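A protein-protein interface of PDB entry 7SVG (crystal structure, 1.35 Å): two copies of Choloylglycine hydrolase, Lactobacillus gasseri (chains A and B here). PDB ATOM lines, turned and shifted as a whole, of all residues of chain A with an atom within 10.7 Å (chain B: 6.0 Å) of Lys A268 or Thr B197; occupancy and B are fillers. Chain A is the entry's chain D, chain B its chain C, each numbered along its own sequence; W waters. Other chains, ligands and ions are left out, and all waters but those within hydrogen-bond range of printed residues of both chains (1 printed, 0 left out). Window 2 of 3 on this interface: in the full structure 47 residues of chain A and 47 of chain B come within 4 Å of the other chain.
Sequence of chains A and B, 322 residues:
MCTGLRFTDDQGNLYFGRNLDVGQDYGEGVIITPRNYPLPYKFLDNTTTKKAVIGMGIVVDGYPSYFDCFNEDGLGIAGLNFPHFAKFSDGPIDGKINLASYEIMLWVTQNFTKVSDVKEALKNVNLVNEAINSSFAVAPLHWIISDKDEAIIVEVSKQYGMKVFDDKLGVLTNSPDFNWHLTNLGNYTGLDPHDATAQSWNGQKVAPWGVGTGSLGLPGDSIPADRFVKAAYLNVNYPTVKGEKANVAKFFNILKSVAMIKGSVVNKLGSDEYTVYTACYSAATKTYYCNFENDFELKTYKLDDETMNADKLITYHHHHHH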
ATOM      1  N   GLY A  23     -29.767 -15.387  26.779  1.00  0.00           N
ATOM      2  CA  GLY A  23     -30.542 -14.515  25.918  1.00  0.00           C
ATOM      3  C   GLY A  23     -31.873 -15.124  25.529  1.00  0.00           C
ATOM      4  O   GLY A  23     -32.780 -14.431  25.058  1.00  0.00           O
ATOM      5  N   ASN A  81     -21.030 -21.027  30.252  1.00  0.00           N
ATOM      6  CA  ASN A  81     -20.667 -20.855  28.846  1.00  0.00           C
ATOM      7  C   ASN A  81     -19.174 -20.557  28.687  1.00  0.00           C
ATOM      8  O   ASN A  81     -18.566 -19.865  29.511  1.00  0.00           O
ATOM      9  CB  ASN A  81     -21.490 -19.722  28.224  1.00  0.00           C
ATOM     10  CG  ASN A  81     -21.717 -19.914  26.729  1.00  0.00           C
ATOM     11  OD1 ASN A  81     -21.804 -21.042  26.236  1.00  0.00           O
ATOM     12  ND2 ASN A  81     -21.810 -18.812  26.002  1.00  0.00           N
ATOM     13  N   PRO A  83     -17.617 -19.841  25.223  1.00  0.00           N
ATOM     14  CA  PRO A  83     -17.622 -19.711  23.766  1.00  0.00           C
ATOM     15  C   PRO A  83     -16.248 -19.306  23.252  1.00  0.00           C
ATOM     16  O   PRO A  83     -15.435 -18.707  23.960  1.00  0.00           O
ATOM     17  CB  PRO A  83     -18.642 -18.590  23.535  1.00  0.00           C
ATOM     18  CG  PRO A  83     -18.500 -17.724  24.774  1.00  0.00           C
ATOM     19  CD  PRO A  83     -18.294 -18.715  25.895  1.00  0.00           C
ATOM     20  N   HIS A  84     -15.986 -19.647  21.991  1.00  0.00           N
ATOM     21  CA  HIS A  84     -14.714 -19.337  21.341  1.00  0.00           C
ATOM     22  C   HIS A  84     -13.544 -20.117  21.914  1.00  0.00           C
ATOM     23  O   HIS A  84     -12.397 -19.844  21.546  1.00  0.00           O
ATOM     24  CB  HIS A  84     -14.389 -17.839  21.384  1.00  0.00           C
ATOM     25  CG  HIS A  84     -15.576 -16.966  21.159  1.00  0.00           C
ATOM     26  ND1 HIS A  84     -16.239 -16.914  19.953  1.00  0.00           N
ATOM     27  CD2 HIS A  84     -16.223 -16.105  21.986  1.00  0.00           C
ATOM     28  CE1 HIS A  84     -17.240 -16.052  20.044  1.00  0.00           C
ATOM     29  NE2 HIS A  84     -17.256 -15.556  21.268  1.00  0.00           N
ATOM     30  N   SER A 264     -29.589  -4.016  29.976  1.00  0.00           N
ATOM     31  CA  SER A 264     -28.257  -3.432  29.944  1.00  0.00           C
ATOM     32  C   SER A 264     -27.315  -4.137  28.968  1.00  0.00           C
ATOM     33  O   SER A 264     -26.239  -3.599  28.685  1.00  0.00           O
ATOM     34  CB  SER A 264     -27.661  -3.425  31.358  1.00  0.00           C
ATOM     35  OG  SER A 264     -27.271  -4.733  31.752  1.00  0.00           O
ATOM     36  N   VAL A 265     -27.683  -5.318  28.463  1.00  0.00           N
ATOM     37  CA  VAL A 265     -26.866  -6.060  27.502  1.00  0.00           C
ATOM     38  C   VAL A 265     -27.777  -6.533  26.374  1.00  0.00           C
ATOM     39  O   VAL A 265     -28.734  -7.278  26.621  1.00  0.00           O
ATOM     40  CB  VAL A 265     -26.183  -7.277  28.154  1.00  0.00           C
ATOM     41  CG1 VAL A 265     -25.323  -8.004  27.116  1.00  0.00           C
ATOM     42  CG2 VAL A 265     -25.335  -6.858  29.360  1.00  0.00           C
ATOM     43  N   VAL A 266     -27.486  -6.114  25.146  1.00  0.00           N
ATOM     44  CA  VAL A 266     -28.193  -6.602  23.963  1.00  0.00           C
ATOM     45  C   VAL A 266     -27.166  -7.268  23.060  1.00  0.00           C
ATOM     46  O   VAL A 266     -26.212  -6.619  22.616  1.00  0.00           O
ATOM     47  CB  VAL A 266     -28.930  -5.476  23.224  1.00  0.00           C
ATOM     48  CG1 VAL A 266     -29.635  -6.015  21.994  1.00  0.00           C
ATOM     49  CG2 VAL A 266     -29.923  -4.795  24.157  1.00  0.00           C
ATOM     50  N   ASN A 267     -27.351  -8.561  22.797  1.00  0.00           N
ATOM     51  CA  ASN A 267     -26.344  -9.280  22.035  1.00  0.00           C
ATOM     52  C   ASN A 267     -26.409  -8.905  20.553  1.00  0.00           C
ATOM     53  O   ASN A 267     -27.290  -8.163  20.103  1.00  0.00           O
ATOM     54  CB  ASN A 267     -26.415 -10.797  22.301  1.00  0.00           C
ATOM     55  CG  ASN A 267     -27.660 -11.463  21.709  1.00  0.00           C
ATOM     56  OD1 ASN A 267     -28.211 -11.017  20.704  1.00  0.00           O
ATOM     57  ND2 ASN A 267     -28.092 -12.555  22.335  1.00  0.00           N
ATOM     58  N   LYS A 268     -25.439  -9.417  19.791  1.00  0.00           N
ATOM     59  CA  LYS A 268     -25.338  -9.056  18.382  1.00  0.00           C
ATOM     60  C   LYS A 268     -26.497  -9.582  17.552  1.00  0.00           C
ATOM     61  O   LYS A 268     -26.689  -9.116  16.424  1.00  0.00           O
ATOM     62  CB  LYS A 268     -24.001  -9.523  17.800  1.00  0.00           C
ATOM     63  CG  LYS A 268     -23.791 -11.026  17.847  1.00  0.00           C
ATOM     64  CD  LYS A 268     -22.441 -11.380  17.229  1.00  0.00           C
ATOM     65  CE  LYS A 268     -22.326 -12.861  16.912  1.00  0.00           C
ATOM     66  NZ  LYS A 268     -22.276 -13.682  18.152  1.00  0.00           N
ATOM     67  N   LEU A 269     -27.269 -10.526  18.080  1.00  0.00           N
ATOM     68  CA  LEU A 269     -28.474 -11.004  17.420  1.00  0.00           C
ATOM     69  C   LEU A 269     -29.727 -10.260  17.865  1.00  0.00           C
ATOM     70  O   LEU A 269     -30.829 -10.630  17.446  1.00  0.00           O
ATOM     71  CB  LEU A 269     -28.638 -12.515  17.641  1.00  0.00           C
ATOM     72  CG  LEU A 269     -27.476 -13.343  17.075  1.00  0.00           C
ATOM     73  CD1 LEU A 269     -27.675 -14.826  17.364  1.00  0.00           C
ATOM     74  CD2 LEU A 269     -27.306 -13.095  15.591  1.00  0.00           C
ATOM     75  N   GLY A 270     -29.591  -9.235  18.713  1.00  0.00           N
ATOM     76  CA  GLY A 270     -30.704  -8.381  19.074  1.00  0.00           C
ATOM     77  C   GLY A 270     -31.445  -8.751  20.340  1.00  0.00           C
ATOM     78  O   GLY A 270     -32.427  -8.078  20.679  1.00  0.00           O
ATOM     79  N   SER A 271     -31.019  -9.784  21.055  1.00  0.00           N
ATOM     80  CA  SER A 271     -31.749 -10.244  22.229  1.00  0.00           C
ATOM     81  C   SER A 271     -31.102  -9.746  23.517  1.00  0.00           C
ATOM     82  O   SER A 271     -29.876  -9.644  23.619  1.00  0.00           O
ATOM     83  CB  SER A 271     -31.830 -11.769  22.263  1.00  0.00           C
ATOM     84  OG  SER A 271     -32.515 -12.257  21.123  1.00  0.00           O
ATOM     85  N   ASP A 272     -31.943  -9.458  24.512  1.00  0.00           N
ATOM     86  CA  ASP A 272     -31.445  -9.102  25.835  1.00  0.00           C
ATOM     87  C   ASP A 272     -30.793 -10.327  26.468  1.00  0.00           C
ATOM     88  O   ASP A 272     -31.370 -11.419  26.467  1.00  0.00           O
ATOM     89  CB  ASP A 272     -32.601  -8.687  26.748  1.00  0.00           C
ATOM     90  CG  ASP A 272     -33.239  -7.365  26.363  1.00  0.00           C
ATOM     91  OD1 ASP A 272     -32.685  -6.615  25.538  1.00  0.00           O
ATOM     92  OD2 ASP A 272     -34.320  -7.075  26.915  1.00  0.00           O
ATOM     93  N   GLU A 273     -29.606 -10.144  27.032  1.00  0.00           N
ATOM     94  CA  GLU A 273     -28.961 -11.162  27.847  1.00  0.00           C
ATOM     95  C   GLU A 273     -29.019 -10.737  29.306  1.00  0.00           C
ATOM     96  O   GLU A 273     -28.705  -9.587  29.634  1.00  0.00           O
ATOM     97  CB  GLU A 273     -27.505 -11.350  27.415  1.00  0.00           C
ATOM     98  CG  GLU A 273     -27.381 -11.770  25.958  1.00  0.00           C
ATOM     99  CD  GLU A 273     -26.836 -13.179  25.784  1.00  0.00           C
ATOM    100  OE1 GLU A 273     -26.508 -13.828  26.801  1.00  0.00           O
ATOM    101  OE2 GLU A 273     -26.710 -13.617  24.619  1.00  0.00           O
ATOM    102  N   ASP B 195     -23.933  -4.917  22.258  1.00  0.00           N
ATOM    103  CA  ASP B 195     -22.586  -5.473  22.212  1.00  0.00           C
ATOM    104  C   ASP B 195     -21.813  -4.924  21.021  1.00  0.00           C
ATOM    105  O   ASP B 195     -22.370  -4.639  19.957  1.00  0.00           O
ATOM    106  CB  ASP B 195     -22.661  -6.993  22.061  1.00  0.00           C
ATOM    107  CG  ASP B 195     -22.967  -7.705  23.361  1.00  0.00           C
ATOM    108  OD1 ASP B 195     -22.913  -7.072  24.443  1.00  0.00           O
ATOM    109  OD2 ASP B 195     -23.276  -8.916  23.287  1.00  0.00           O
ATOM    110  N   ALA B 196     -20.504  -4.799  21.203  1.00  0.00           N
ATOM    111  CA  ALA B 196     -19.629  -4.588  20.068  1.00  0.00           C
ATOM    112  C   ALA B 196     -19.542  -5.884  19.267  1.00  0.00           C
ATOM    113  O   ALA B 196     -19.994  -6.946  19.702  1.00  0.00           O
ATOM    114  CB  ALA B 196     -18.249  -4.146  20.554  1.00  0.00           C
ATOM    115  N   THR B 197     -18.963  -5.804  18.076  1.00  0.00           N
ATOM    116  CA  THR B 197     -18.719  -6.996  17.277  1.00  0.00           C
ATOM    117  C   THR B 197     -17.259  -7.016  16.857  1.00  0.00           C
ATOM    118  O   THR B 197     -16.480  -6.124  17.208  1.00  0.00           O
ATOM    119  CB  THR B 197     -19.664  -7.083  16.070  1.00  0.00           C
ATOM    120  OG1 THR B 197     -19.544  -5.900  15.272  1.00  0.00           O
ATOM    121  CG2 THR B 197     -21.114  -7.255  16.539  1.00  0.00           C
ATOM    122  N   ALA B 198     -16.902  -8.047  16.092  1.00  0.00           N
ATOM    123  CA  ALA B 198     -15.511  -8.267  15.722  1.00  0.00           C
ATOM    124  C   ALA B 198     -14.977  -7.094  14.912  1.00  0.00           C
ATOM    125  O   ALA B 198     -15.677  -6.528  14.068  1.00  0.00           O
ATOM    126  CB  ALA B 198     -15.394  -9.562  14.913  1.00  0.00           C
ATOM    127  N   GLN B 199     -13.713  -6.751  15.154  1.00  0.00           N
ATOM    128  CA  GLN B 199     -13.062  -5.620  14.517  1.00  0.00           C
ATOM    129  C   GLN B 199     -11.735  -6.063  13.919  1.00  0.00           C
ATOM    130  O   GLN B 199     -11.204  -7.127  14.250  1.00  0.00           O
ATOM    131  CB  GLN B 199     -12.827  -4.500  15.533  1.00  0.00           C
ATOM    132  CG  GLN B 199     -14.137  -3.957  16.075  1.00  0.00           C
ATOM    133  CD  GLN B 199     -13.987  -3.210  17.387  1.00  0.00           C
ATOM    134  OE1 GLN B 199     -12.878  -2.913  17.832  1.00  0.00           O
ATOM    135  NE2 GLN B 199     -15.119  -2.870  18.000  1.00  0.00           N
ATOM    136  N   VAL B 206      -9.817  -8.605  16.330  1.00  0.00           N
ATOM    137  CA  VAL B 206     -10.071  -8.298  17.731  1.00  0.00           C
ATOM    138  C   VAL B 206     -11.571  -8.434  17.928  1.00  0.00           C
ATOM    139  O   VAL B 206     -12.345  -7.617  17.411  1.00  0.00           O
ATOM    140  CB  VAL B 206      -9.601  -6.880  18.080  1.00  0.00           C
ATOM    141  CG1 VAL B 206      -9.975  -6.526  19.515  1.00  0.00           C
ATOM    142  CG2 VAL B 206      -8.101  -6.755  17.874  1.00  0.00           C
ATOM    143  N   ALA B 207     -11.987  -9.453  18.672  1.00  0.00           N
ATOM    144  CA  ALA B 207     -13.409  -9.729  18.785  1.00  0.00           C
ATOM    145  C   ALA B 207     -13.788  -9.982  20.234  1.00  0.00           C
ATOM    146  O   ALA B 207     -12.968 -10.461  21.025  1.00  0.00           O
ATOM    147  CB  ALA B 207     -13.803 -10.946  17.944  1.00  0.00           C
ATOM    148  N   PRO B 208     -15.026  -9.666  20.607  1.00  0.00           N
ATOM    149  CA  PRO B 208     -15.472  -9.928  21.983  1.00  0.00           C
ATOM    150  C   PRO B 208     -15.363 -11.396  22.359  1.00  0.00           C
ATOM    151  O   PRO B 208     -15.561 -12.293  21.535  1.00  0.00           O
ATOM    152  CB  PRO B 208     -16.940  -9.488  21.973  1.00  0.00           C
ATOM    153  CG  PRO B 208     -17.042  -8.520  20.853  1.00  0.00           C
ATOM    154  CD  PRO B 208     -16.055  -8.981  19.809  1.00  0.00           C
ATOM    155  N   THR B 213     -19.893  -5.984  26.040  1.00  0.00           N
ATOM    156  CA  THR B 213     -18.793  -5.101  25.659  1.00  0.00           C
ATOM    157  C   THR B 213     -19.208  -3.642  25.449  1.00  0.00           C
ATOM    158  O   THR B 213     -18.345  -2.759  25.520  1.00  0.00           O
ATOM    159  CB  THR B 213     -18.105  -5.641  24.402  1.00  0.00           C
ATOM    160  OG1 THR B 213     -19.096  -5.951  23.414  1.00  0.00           O
ATOM    161  CG2 THR B 213     -17.331  -6.906  24.733  1.00  0.00           C
HETATM  162  O   HOH W   1     -23.081 -10.390  21.097  1.00  0.00           O
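The backbone NH (N) of Asp B195 is in hydrogen-bond range of the backbone carbonyl oxygen (O) of Val A266, at 2.9 Å.
The backbone carbonyl oxygen of Val A265 is in hydrogen-bond range of the backbone NH of Glu A273 (3.0 Å). OD1 of Asn A267 sits at hydrogen-bond distance from N of Leu A269 (2.8 Å). The backbone NH (N) of Ser A271 lies within hydrogen-bond range of the side-chain amide oxygen (OD1) of Asn A267 (3.1 Å). ND2 of Asn A267 lies within hydrogen-bond range of OE2 of Glu A273 (2.9 Å). The side-chain amide oxygen of Asn A267 sits at hydrogen-bond distance from the backbone NH of Gly A270 (3.0 Å).
Pro B208 touches His A84 (O to NE2, 3.7 Å). CG1 of Val A265 touches OD1 of Asp B195, at 3.7 Å. Asp B195 touches Asn A267. Lys A268 touches Thr B197.
Printed residues of chain B within 4 Å of His A84: Pro B208 (3.7 Å). Of the printed residues of chain B, Asn A267 touches Asp B195. Asp B195 touches just these residues of chain A: Val A265 (3.7 Å), Val A266 (2.9 Å) and Asn A267 (3.3 Å). No residue of chain A comes within 4 Å of Ala B196. No residue of chain A comes within 4 Å of Gln B199. Val B206 touches none of the printed residues of chain A. The nearest residue of chain B that does not touch Lys A268 is Asp B195 (4.1 Å). The nearest residue of chain A that does not touch Thr B197 is Asn A267 (6.8 Å). The nearest printed residue of chain B that does not touch Val A265 is Thr B213 (5.9 Å).
No position is printed for both chains.
Water W1 lies within hydrogen-bond range of OD2 of Asp B195 (2.6 Å) and N of Lys A268 (2.9 Å).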
